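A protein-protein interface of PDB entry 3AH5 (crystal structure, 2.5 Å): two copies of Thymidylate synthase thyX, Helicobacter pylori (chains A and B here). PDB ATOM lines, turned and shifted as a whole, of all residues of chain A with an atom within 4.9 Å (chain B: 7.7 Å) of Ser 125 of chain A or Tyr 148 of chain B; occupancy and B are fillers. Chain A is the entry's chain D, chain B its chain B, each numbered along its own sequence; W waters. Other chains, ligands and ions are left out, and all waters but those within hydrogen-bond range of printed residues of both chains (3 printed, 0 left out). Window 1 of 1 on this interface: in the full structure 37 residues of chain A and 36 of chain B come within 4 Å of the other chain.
The backbone carbonyl oxygen (O) of Tyr 148 of chain B lies close to the side-chain hydroxyl (OG) of Ser 153 of chain A, at 3.1 Å.
The side-chain amide oxygen (OD1) of Asn 131 of chain B lies close to the side-chain sulfur (SD) of Met 124 of chain A.
The backbone carbonyl oxygen (O) of Met 150 of chain B is in hydrogen-bond range of the backbone NH (N) of Glu 152 of chain A, 2.9 Å away.
The side-chain carboxylate (OE2) of Glu 182 of chain A lies within hydrogen-bond range of the side-chain hydroxyl (OH) of Tyr 148 of chain B (2.5 Å).
The side-chain hydroxyl of Ser 125 of chain A lies within hydrogen-bond range of the backbone carbonyl oxygen of Tyr 148 of chain B (3.5 Å).
OG of Ser 125 of chain A lies within hydrogen-bond range of OG of Ser 153 of chain A, at 3.1 Å.
N of Val 114 of chain A sits at hydrogen-bond distance from O of Ser 153 of chain A (2.8 Å).
The side-chain hydroxyl of Ser 65 of chain A sits at hydrogen-bond distance from the side-chain carboxylate of Glu 182 of chain A.
NZ of Lys 147 of chain B sits at hydrogen-bond distance from OG of Ser 85 of chain B, at 3.0 Å.
The backbone carbonyl oxygen (O) of Val 121 of chain A lies within hydrogen-bond range of the side-chain hydroxyl (OG) of Ser 125 of chain A, 3.1 Å away.
The backbone NH (N) of Val 116 of chain A sits at hydrogen-bond distance from the side-chain amide oxygen (OD1) of Asn 122 of chain A, 2.7 Å away.
Among the printed residues, pairs that only touch across the chains: Ser 65 of chain A with Tyr 148 of chain B (3.5 Å), Val 116 of chain A with Tyr 148 of chain B (3.6 Å), Val 121 of chain A with Leu 135 of chain B (3.8 Å), Met 124 of chain A with Leu 135 of chain B (3.5 Å), Pro 151 of chain A with Met 150 of chain B (3.5 Å), Glu 152 of chain A with Tyr 148 of chain B (3.9 Å), Leu 180 of chain A with Asp 144 of chain B (3.7 Å), Leu 180 of chain A with Lys 147 of chain B (3.7 Å) and Leu 180 of chain A with Tyr 148 of chain B (3.8 Å).
Printed residues of chain B within 4 Å of Ser 65 of chain A: Tyr 148 (3.5 Å).
Of the printed residues of chain B, Val 116 of chain A touches Tyr 148.
Ser 125 of chain A touches just one residue of chain B: Tyr 148.
Of the printed residues of chain B, Pro 151 of chain A touches Met 150.
Printed residues of chain B within 4 Å of Leu 180 of chain A: Asp 144 (3.7 Å), Lys 147 (3.7 Å) and Tyr 148 (3.8 Å).
Tyr 148 of chain B touches just these residues of chain A: Ser 65, Val 116, Ser 125, Glu 152, Ser 153, Leu 180 and Glu 182.
The nearest residue of chain B that does not touch Ser 125 of chain A is Ala 149 of chain B (4.1 Å).
The nearest residue of chain A that does not touch Tyr 148 of chain B is Pro 151 of chain A (4.03 Å).
The nearest printed residue of chain A that does not touch Asn 131 of chain B is Leu 127 of chain A (4.3 Å).
Of the 15 printed residues of chain B, 6 touch a printed residue of chain A.
Printed residues of chain B that touch a printed residue of chain A: Asn 131, Leu 135, Asp 144, Lys 147, Tyr 148 and Met 150.
Of the 18 printed residues of chain A, 10 touch a printed residue of chain B.
Hydrophobic or aromatic side chains of chain A within 4 Å of the printed part of chain B: Val 116, Val 121, Met 124 and Leu 180.
Among the printed residues, 14 pairs touch across the chains.
Among the printed residues, no Asp or Glu carboxylate lies within 4 Å of a Lys or Arg side-chain nitrogen of the other chain.
1 position is printed for both chains.
Water W3 bridges the side-chain hydroxyl of Tyr 148 of chain B (2.5 Å) and the backbone NH of Glu 182 of chain A (3.1 Å).
Water W1 bridges the side-chain carboxylate of Glu 152 of chain A (2.5 Å) and the backbone carbonyl oxygen of Lys 147 of chain B (2.7 Å).
Water W2 lies within hydrogen-bond range of the backbone carbonyl oxygen of Met 124 of chain A (2.5 Å) and the side-chain amide nitrogen of Asn 131 of chain B (2.9 Å).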
ATOM      1  N   SER A  65     -22.874  -5.618 -26.445  1.00  0.00           N
ATOM      2  CA  SER A  65     -22.791  -5.578 -24.984  1.00  0.00           C
ATOM      3  C   SER A  65     -21.989  -6.758 -24.419  1.00  0.00           C
ATOM      4  O   SER A  65     -21.808  -7.780 -25.087  1.00  0.00           O
ATOM      5  CB  SER A  65     -24.190  -5.586 -24.367  1.00  0.00           C
ATOM      6  OG  SER A  65     -24.758  -6.875 -24.424  1.00  0.00           O
ATOM      7  N   LEU A 113     -22.110   2.392 -23.302  1.00  0.00           N
ATOM      8  CA  LEU A 113     -23.150   1.442 -22.944  1.00  0.00           C
ATOM      9  C   LEU A 113     -24.066   1.099 -24.090  1.00  0.00           C
ATOM     10  O   LEU A 113     -24.209   1.867 -25.038  1.00  0.00           O
ATOM     11  CB  LEU A 113     -24.012   1.993 -21.809  1.00  0.00           C
ATOM     12  CG  LEU A 113     -23.385   2.421 -20.485  1.00  0.00           C
ATOM     13  CD1 LEU A 113     -24.471   3.022 -19.595  1.00  0.00           C
ATOM     14  CD2 LEU A 113     -22.736   1.237 -19.805  1.00  0.00           C
ATOM     15  N   VAL A 114     -24.676  -0.076 -23.991  1.00  0.00           N
ATOM     16  CA  VAL A 114     -25.644  -0.527 -24.969  1.00  0.00           C
ATOM     17  C   VAL A 114     -26.960  -0.232 -24.275  1.00  0.00           C
ATOM     18  O   VAL A 114     -27.145  -0.599 -23.112  1.00  0.00           O
ATOM     19  CB  VAL A 114     -25.574  -2.047 -25.224  1.00  0.00           C
ATOM     20  CG1 VAL A 114     -26.727  -2.468 -26.135  1.00  0.00           C
ATOM     21  CG2 VAL A 114     -24.248  -2.417 -25.860  1.00  0.00           C
ATOM     22  N   VAL A 116     -31.234  -0.448 -24.067  1.00  0.00           N
ATOM     23  CA  VAL A 116     -32.300  -1.380 -24.403  1.00  0.00           C
ATOM     24  C   VAL A 116     -33.666  -0.699 -24.359  1.00  0.00           C
ATOM     25  O   VAL A 116     -33.779   0.476 -24.009  1.00  0.00           O
ATOM     26  CB  VAL A 116     -32.313  -2.589 -23.432  1.00  0.00           C
ATOM     27  CG1 VAL A 116     -30.958  -3.294 -23.455  1.00  0.00           C
ATOM     28  CG2 VAL A 116     -32.650  -2.126 -22.027  1.00  0.00           C
ATOM     29  N   VAL A 121     -34.035   0.771 -16.943  1.00  0.00           N
ATOM     30  CA  VAL A 121     -32.864  -0.089 -16.900  1.00  0.00           C
ATOM     31  C   VAL A 121     -31.664   0.632 -17.515  1.00  0.00           C
ATOM     32  O   VAL A 121     -30.527   0.408 -17.103  1.00  0.00           O
ATOM     33  CB  VAL A 121     -33.117  -1.447 -17.627  1.00  0.00           C
ATOM     34  CG1 VAL A 121     -34.459  -2.027 -17.199  1.00  0.00           C
ATOM     35  CG2 VAL A 121     -33.075  -1.270 -19.112  1.00  0.00           C
ATOM     36  N   ASN A 122     -31.917   1.502 -18.490  1.00  0.00           N
ATOM     37  CA  ASN A 122     -30.829   2.248 -19.122  1.00  0.00           C
ATOM     38  C   ASN A 122     -30.266   3.245 -18.121  1.00  0.00           C
ATOM     39  O   ASN A 122     -29.056   3.456 -18.049  1.00  0.00           O
ATOM     40  CB  ASN A 122     -31.320   3.006 -20.357  1.00  0.00           C
ATOM     41  CG  ASN A 122     -31.803   2.084 -21.452  1.00  0.00           C
ATOM     42  OD1 ASN A 122     -31.108   1.149 -21.843  1.00  0.00           O
ATOM     43  ND2 ASN A 122     -33.001   2.348 -21.961  1.00  0.00           N
ATOM     44  N   ALA A 123     -31.161   3.865 -17.357  1.00  0.00           N
ATOM     45  CA  ALA A 123     -30.756   4.830 -16.346  1.00  0.00           C
ATOM     46  C   ALA A 123     -29.874   4.125 -15.323  1.00  0.00           C
ATOM     47  O   ALA A 123     -28.804   4.619 -14.955  1.00  0.00           O
ATOM     48  CB  ALA A 123     -31.987   5.414 -15.660  1.00  0.00           C
ATOM     49  N   MET A 124     -30.331   2.962 -14.870  1.00  0.00           N
ATOM     50  CA  MET A 124     -29.591   2.180 -13.892  1.00  0.00           C
ATOM     51  C   MET A 124     -28.216   1.786 -14.427  1.00  0.00           C
ATOM     52  O   MET A 124     -27.272   1.596 -13.657  1.00  0.00           O
ATOM     53  CB  MET A 124     -30.391   0.932 -13.507  1.00  0.00           C
ATOM     54  CG  MET A 124     -31.693   1.230 -12.767  1.00  0.00           C
ATOM     55  SD  MET A 124     -31.453   2.077 -11.174  1.00  0.00           S
ATOM     56  CE  MET A 124     -31.844   3.761 -11.615  1.00  0.00           C
ATOM     57  N   SER A 125     -28.104   1.664 -15.745  1.00  0.00           N
ATOM     58  CA  SER A 125     -26.828   1.316 -16.362  1.00  0.00           C
ATOM     59  C   SER A 125     -25.873   2.504 -16.264  1.00  0.00           C
ATOM     60  O   SER A 125     -24.696   2.345 -15.934  1.00  0.00           O
ATOM     61  CB  SER A 125     -27.014   0.936 -17.837  1.00  0.00           C
ATOM     62  OG  SER A 125     -27.654  -0.321 -17.983  1.00  0.00           O
ATOM     63  N   VAL A 126     -26.387   3.696 -16.549  1.00  0.00           N
ATOM     64  CA  VAL A 126     -25.563   4.893 -16.495  1.00  0.00           C
ATOM     65  C   VAL A 126     -25.089   5.101 -15.063  1.00  0.00           C
ATOM     66  O   VAL A 126     -23.936   5.454 -14.825  1.00  0.00           O
ATOM     67  CB  VAL A 126     -26.346   6.134 -17.001  1.00  0.00           C
ATOM     68  CG1 VAL A 126     -25.461   7.356 -16.969  1.00  0.00           C
ATOM     69  CG2 VAL A 126     -26.840   5.891 -18.425  1.00  0.00           C
ATOM     70  N   LEU A 127     -25.974   4.877 -14.103  1.00  0.00           N
ATOM     71  CA  LEU A 127     -25.589   5.030 -12.709  1.00  0.00           C
ATOM     72  C   LEU A 127     -24.435   4.060 -12.431  1.00  0.00           C
ATOM     73  O   LEU A 127     -23.462   4.412 -11.760  1.00  0.00           O
ATOM     74  CB  LEU A 127     -26.783   4.742 -11.792  1.00  0.00           C
ATOM     75  CG  LEU A 127     -27.529   5.958 -11.211  1.00  0.00           C
ATOM     76  CD1 LEU A 127     -27.918   6.925 -12.311  1.00  0.00           C
ATOM     77  CD2 LEU A 127     -28.766   5.478 -10.459  1.00  0.00           C
ATOM     78  N   ALA A 128     -24.537   2.843 -12.965  1.00  0.00           N
ATOM     79  CA  ALA A 128     -23.483   1.849 -12.788  1.00  0.00           C
ATOM     80  C   ALA A 128     -22.212   2.319 -13.492  1.00  0.00           C
ATOM     81  O   ALA A 128     -21.100   2.081 -13.019  1.00  0.00           O
ATOM     82  CB  ALA A 128     -23.919   0.519 -13.357  1.00  0.00           C
ATOM     83  N   LEU A 129     -22.384   2.981 -14.631  1.00  0.00           N
ATOM     84  CA  LEU A 129     -21.258   3.497 -15.400  1.00  0.00           C
ATOM     85  C   LEU A 129     -20.565   4.625 -14.642  1.00  0.00           C
ATOM     86  O   LEU A 129     -19.340   4.734 -14.661  1.00  0.00           O
ATOM     87  CB  LEU A 129     -21.739   4.019 -16.755  1.00  0.00           C
ATOM     88  CG  LEU A 129     -20.686   4.728 -17.612  1.00  0.00           C
ATOM     89  CD1 LEU A 129     -19.622   3.728 -18.054  1.00  0.00           C
ATOM     90  CD2 LEU A 129     -21.355   5.368 -18.819  1.00  0.00           C
ATOM     91  N   PRO A 151     -21.215  -2.743 -15.440  1.00  0.00           N
ATOM     92  CA  PRO A 151     -22.516  -3.300 -15.814  1.00  0.00           C
ATOM     93  C   PRO A 151     -22.372  -4.098 -17.107  1.00  0.00           C
ATOM     94  O   PRO A 151     -21.589  -3.725 -17.982  1.00  0.00           O
ATOM     95  CB  PRO A 151     -23.371  -2.056 -15.987  1.00  0.00           C
ATOM     96  CG  PRO A 151     -22.400  -1.092 -16.599  1.00  0.00           C
ATOM     97  CD  PRO A 151     -21.135  -1.310 -15.788  1.00  0.00           C
ATOM     98  N   GLU A 152     -23.126  -5.187 -17.238  1.00  0.00           N
ATOM     99  CA  GLU A 152     -23.024  -6.016 -18.437  1.00  0.00           C
ATOM    100  C   GLU A 152     -23.478  -5.327 -19.720  1.00  0.00           C
ATOM    101  O   GLU A 152     -23.336  -5.881 -20.808  1.00  0.00           O
ATOM    102  CB  GLU A 152     -23.789  -7.326 -18.252  1.00  0.00           C
ATOM    103  CG  GLU A 152     -23.180  -8.251 -17.209  1.00  0.00           C
ATOM    104  CD  GLU A 152     -23.114  -9.694 -17.680  1.00  0.00           C
ATOM    105  OE1 GLU A 152     -24.015 -10.120 -18.430  1.00  0.00           O
ATOM    106  OE2 GLU A 152     -22.165 -10.406 -17.291  1.00  0.00           O
ATOM    107  N   SER A 153     -24.015  -4.118 -19.596  1.00  0.00           N
ATOM    108  CA  SER A 153     -24.447  -3.365 -20.771  1.00  0.00           C
ATOM    109  C   SER A 153     -23.258  -2.580 -21.349  1.00  0.00           C
ATOM    110  O   SER A 153     -23.385  -1.909 -22.365  1.00  0.00           O
ATOM    111  CB  SER A 153     -25.594  -2.401 -20.414  1.00  0.00           C
ATOM    112  OG  SER A 153     -25.193  -1.435 -19.457  1.00  0.00           O
ATOM    113  N   LEU A 180     -31.872 -14.178 -26.746  1.00  0.00           N
ATOM    114  CA  LEU A 180     -31.899 -12.805 -26.248  1.00  0.00           C
ATOM    115  C   LEU A 180     -31.975 -11.882 -27.463  1.00  0.00           C
ATOM    116  O   LEU A 180     -31.285 -12.111 -28.458  1.00  0.00           O
ATOM    117  CB  LEU A 180     -30.623 -12.515 -25.455  1.00  0.00           C
ATOM    118  CG  LEU A 180     -30.401 -11.088 -24.955  1.00  0.00           C
ATOM    119  CD1 LEU A 180     -31.468 -10.715 -23.948  1.00  0.00           C
ATOM    120  CD2 LEU A 180     -29.020 -10.993 -24.327  1.00  0.00           C
ATOM    121  N   GLU A 182     -30.737  -8.998 -28.397  1.00  0.00           N
ATOM    122  CA  GLU A 182     -29.479  -8.526 -28.973  1.00  0.00           C
ATOM    123  C   GLU A 182     -28.783  -9.585 -29.835  1.00  0.00           C
ATOM    124  O   GLU A 182     -28.160  -9.263 -30.857  1.00  0.00           O
ATOM    125  CB  GLU A 182     -28.526  -8.059 -27.869  1.00  0.00           C
ATOM    126  CG  GLU A 182     -27.331  -7.277 -28.392  1.00  0.00           C
ATOM    127  CD  GLU A 182     -26.427  -6.765 -27.286  1.00  0.00           C
ATOM    128  OE1 GLU A 182     -25.448  -6.061 -27.608  1.00  0.00           O
ATOM    129  OE2 GLU A 182     -26.685  -7.070 -26.102  1.00  0.00           O
ATOM    130  N   SER B  85     -28.932 -15.965 -16.300  1.00  0.00           N
ATOM    131  CA  SER B  85     -29.471 -14.743 -15.722  1.00  0.00           C
ATOM    132  C   SER B  85     -30.827 -14.502 -16.371  1.00  0.00           C
ATOM    133  O   SER B  85     -31.764 -14.043 -15.727  1.00  0.00           O
ATOM    134  CB  SER B  85     -28.544 -13.548 -15.986  1.00  0.00           C
ATOM    135  OG  SER B  85     -28.495 -13.206 -17.362  1.00  0.00           O
ATOM    136  N   LEU B  89     -33.054 -14.472 -12.854  1.00  0.00           N
ATOM    137  CA  LEU B  89     -32.956 -13.202 -12.156  1.00  0.00           C
ATOM    138  C   LEU B  89     -34.083 -12.900 -11.169  1.00  0.00           C
ATOM    139  O   LEU B  89     -33.927 -12.037 -10.310  1.00  0.00           O
ATOM    140  CB  LEU B  89     -32.815 -12.055 -13.154  1.00  0.00           C
ATOM    141  CG  LEU B  89     -31.348 -11.667 -13.348  1.00  0.00           C
ATOM    142  CD1 LEU B  89     -31.246 -10.450 -14.269  1.00  0.00           C
ATOM    143  CD2 LEU B  89     -30.719 -11.366 -11.980  1.00  0.00           C
ATOM    144  N   ASN B 131     -29.796  -1.564  -7.414  1.00  0.00           N
ATOM    145  CA  ASN B 131     -30.554  -1.011  -8.532  1.00  0.00           C
ATOM    146  C   ASN B 131     -31.105  -2.116  -9.421  1.00  0.00           C
ATOM    147  O   ASN B 131     -32.147  -1.948 -10.059  1.00  0.00           O
ATOM    148  CB  ASN B 131     -29.692  -0.058  -9.366  1.00  0.00           C
ATOM    149  CG  ASN B 131     -29.398   1.241  -8.643  1.00  0.00           C
ATOM    150  OD1 ASN B 131     -30.293   1.862  -8.072  1.00  0.00           O
ATOM    151  ND2 ASN B 131     -28.144   1.666  -8.672  1.00  0.00           N
ATOM    152  N   LEU B 132     -30.405  -3.246  -9.469  1.00  0.00           N
ATOM    153  CA  LEU B 132     -30.860  -4.366 -10.280  1.00  0.00           C
ATOM    154  C   LEU B 132     -32.070  -4.986  -9.603  1.00  0.00           C
ATOM    155  O   LEU B 132     -33.022  -5.399 -10.268  1.00  0.00           O
ATOM    156  CB  LEU B 132     -29.759  -5.420 -10.420  1.00  0.00           C
ATOM    157  CG  LEU B 132     -30.162  -6.719 -11.132  1.00  0.00           C
ATOM    158  CD1 LEU B 132     -30.558  -6.439 -12.579  1.00  0.00           C
ATOM    159  CD2 LEU B 132     -29.005  -7.697 -11.081  1.00  0.00           C
ATOM    160  N   LEU B 135     -35.201  -2.877 -10.322  1.00  0.00           N
ATOM    161  CA  LEU B 135     -35.756  -3.050 -11.659  1.00  0.00           C
ATOM    162  C   LEU B 135     -36.633  -4.297 -11.707  1.00  0.00           C
ATOM    163  O   LEU B 135     -37.678  -4.324 -12.368  1.00  0.00           O
ATOM    164  CB  LEU B 135     -34.631  -3.208 -12.684  1.00  0.00           C
ATOM    165  CG  LEU B 135     -33.648  -2.061 -12.925  1.00  0.00           C
ATOM    166  CD1 LEU B 135     -32.551  -2.535 -13.871  1.00  0.00           C
ATOM    167  CD2 LEU B 135     -34.376  -0.868 -13.519  1.00  0.00           C
ATOM    168  N   LYS B 142     -38.828  -7.462 -17.065  1.00  0.00           N
ATOM    169  CA  LYS B 142     -38.348  -8.751 -17.547  1.00  0.00           C
ATOM    170  C   LYS B 142     -36.848  -8.977 -17.390  1.00  0.00           C
ATOM    171  O   LYS B 142     -36.058  -8.033 -17.363  1.00  0.00           O
ATOM    172  CB  LYS B 142     -38.762  -8.936 -19.008  1.00  0.00           C
ATOM    173  CG  LYS B 142     -40.185  -9.446 -19.139  1.00  0.00           C
ATOM    174  CD  LYS B 142     -40.649  -9.538 -20.583  1.00  0.00           C
ATOM    175  CE  LYS B 142     -41.874 -10.453 -20.695  1.00  0.00           C
ATOM    176  NZ  LYS B 142     -42.944 -10.112 -19.706  1.00  0.00           N
ATOM    177  N   ASN B 143     -36.456 -10.243 -17.281  1.00  0.00           N
ATOM    178  CA  ASN B 143     -35.049 -10.578 -17.120  1.00  0.00           C
ATOM    179  C   ASN B 143     -34.189 -10.128 -18.293  1.00  0.00           C
ATOM    180  O   ASN B 143     -33.118  -9.555 -18.095  1.00  0.00           O
ATOM    181  CB  ASN B 143     -34.872 -12.080 -16.906  1.00  0.00           C
ATOM    182  CG  ASN B 143     -35.454 -12.552 -15.591  1.00  0.00           C
ATOM    183  OD1 ASN B 143     -35.529 -11.792 -14.623  1.00  0.00           O
ATOM    184  ND2 ASN B 143     -35.852 -13.819 -15.542  1.00  0.00           N
ATOM    185  N   ASP B 144     -34.654 -10.380 -19.511  1.00  0.00           N
ATOM    186  CA  ASP B 144     -33.899  -9.999 -20.699  1.00  0.00           C
ATOM    187  C   ASP B 144     -33.534  -8.514 -20.758  1.00  0.00           C
ATOM    188  O   ASP B 144     -32.598  -8.126 -21.456  1.00  0.00           O
ATOM    189  CB  ASP B 144     -34.664 -10.410 -21.961  1.00  0.00           C
ATOM    190  CG  ASP B 144     -34.573 -11.911 -22.234  1.00  0.00           C
ATOM    191  OD1 ASP B 144     -34.027 -12.640 -21.379  1.00  0.00           O
ATOM    192  OD2 ASP B 144     -35.043 -12.363 -23.299  1.00  0.00           O
ATOM    193  N   LEU B 145     -34.263  -7.682 -20.026  1.00  0.00           N
ATOM    194  CA  LEU B 145     -33.976  -6.252 -20.018  1.00  0.00           C
ATOM    195  C   LEU B 145     -33.157  -5.880 -18.781  1.00  0.00           C
ATOM    196  O   LEU B 145     -32.103  -5.256 -18.886  1.00  0.00           O
ATOM    197  CB  LEU B 145     -35.280  -5.443 -20.050  1.00  0.00           C
ATOM    198  CG  LEU B 145     -36.177  -5.610 -21.287  1.00  0.00           C
ATOM    199  CD1 LEU B 145     -37.423  -4.751 -21.128  1.00  0.00           C
ATOM    200  CD2 LEU B 145     -35.427  -5.213 -22.547  1.00  0.00           C
ATOM    201  N   ALA B 146     -33.640  -6.284 -17.615  1.00  0.00           N
ATOM    202  CA  ALA B 146     -32.968  -5.992 -16.354  1.00  0.00           C
ATOM    203  C   ALA B 146     -31.531  -6.504 -16.298  1.00  0.00           C
ATOM    204  O   ALA B 146     -30.687  -5.922 -15.608  1.00  0.00           O
ATOM    205  CB  ALA B 146     -33.774  -6.578 -15.187  1.00  0.00           C
ATOM    206  N   LYS B 147     -31.246  -7.586 -17.019  1.00  0.00           N
ATOM    207  CA  LYS B 147     -29.901  -8.149 -17.008  1.00  0.00           C
ATOM    208  C   LYS B 147     -28.824  -7.158 -17.443  1.00  0.00           C
ATOM    209  O   LYS B 147     -27.663  -7.296 -17.061  1.00  0.00           O
ATOM    210  CB  LYS B 147     -29.833  -9.420 -17.872  1.00  0.00           C
ATOM    211  CG  LYS B 147     -30.253  -9.247 -19.328  1.00  0.00           C
ATOM    212  CD  LYS B 147     -30.228 -10.578 -20.093  1.00  0.00           C
ATOM    213  CE  LYS B 147     -28.826 -10.978 -20.584  1.00  0.00           C
ATOM    214  NZ  LYS B 147     -27.827 -11.255 -19.504  1.00  0.00           N
ATOM    215  N   TYR B 148     -29.196  -6.144 -18.215  1.00  0.00           N
ATOM    216  CA  TYR B 148     -28.199  -5.176 -18.668  1.00  0.00           C
ATOM    217  C   TYR B 148     -27.634  -4.265 -17.580  1.00  0.00           C
ATOM    218  O   TYR B 148     -26.615  -3.612 -17.798  1.00  0.00           O
ATOM    219  CB  TYR B 148     -28.746  -4.330 -19.826  1.00  0.00           C
ATOM    220  CG  TYR B 148     -28.774  -5.071 -21.142  1.00  0.00           C
ATOM    221  CD1 TYR B 148     -29.702  -6.091 -21.369  1.00  0.00           C
ATOM    222  CD2 TYR B 148     -27.846  -4.788 -22.144  1.00  0.00           C
ATOM    223  CE1 TYR B 148     -29.704  -6.819 -22.569  1.00  0.00           C
ATOM    224  CE2 TYR B 148     -27.837  -5.512 -23.350  1.00  0.00           C
ATOM    225  CZ  TYR B 148     -28.770  -6.525 -23.548  1.00  0.00           C
ATOM    226  OH  TYR B 148     -28.778  -7.246 -24.710  1.00  0.00           O
ATOM    227  N   ALA B 149     -28.276  -4.234 -16.413  1.00  0.00           N
ATOM    228  CA  ALA B 149     -27.809  -3.397 -15.304  1.00  0.00           C
ATOM    229  C   ALA B 149     -27.097  -4.235 -14.249  1.00  0.00           C
ATOM    230  O   ALA B 149     -26.817  -3.768 -13.144  1.00  0.00           O
ATOM    231  CB  ALA B 149     -28.989  -2.656 -14.667  1.00  0.00           C
ATOM    232  N   MET B 150     -26.794  -5.477 -14.596  1.00  0.00           N
ATOM    233  CA  MET B 150     -26.132  -6.383 -13.672  1.00  0.00           C
ATOM    234  C   MET B 150     -24.614  -6.202 -13.644  1.00  0.00           C
ATOM    235  O   MET B 150     -23.950  -6.258 -14.678  1.00  0.00           O
ATOM    236  CB  MET B 150     -26.490  -7.831 -14.041  1.00  0.00           C
ATOM    237  CG  MET B 150     -25.880  -8.895 -13.136  1.00  0.00           C
ATOM    238  SD  MET B 150     -26.413 -10.570 -13.595  1.00  0.00           S
ATOM    239  CE  MET B 150     -25.945 -10.610 -15.341  1.00  0.00           C
ATOM    240  N   PRO B 151     -24.045  -5.976 -12.454  1.00  0.00           N
ATOM    241  CA  PRO B 151     -22.594  -5.795 -12.322  1.00  0.00           C
ATOM    242  C   PRO B 151     -21.900  -7.134 -12.598  1.00  0.00           C
ATOM    243  O   PRO B 151     -22.444  -8.191 -12.280  1.00  0.00           O
ATOM    244  CB  PRO B 151     -22.440  -5.355 -10.875  1.00  0.00           C
ATOM    245  CG  PRO B 151     -23.525  -6.140 -10.188  1.00  0.00           C
ATOM    246  CD  PRO B 151     -24.700  -5.955 -11.133  1.00  0.00           C
HETATM  247  O   HOH W   1     -26.282  -9.120 -18.558  1.00  0.00           O
HETATM  248  O   HOH W   2     -27.027   0.925 -11.248  1.00  0.00           O
HETATM  249  O   HOH W   3     -31.016  -7.679 -25.657  1.00  0.00           O
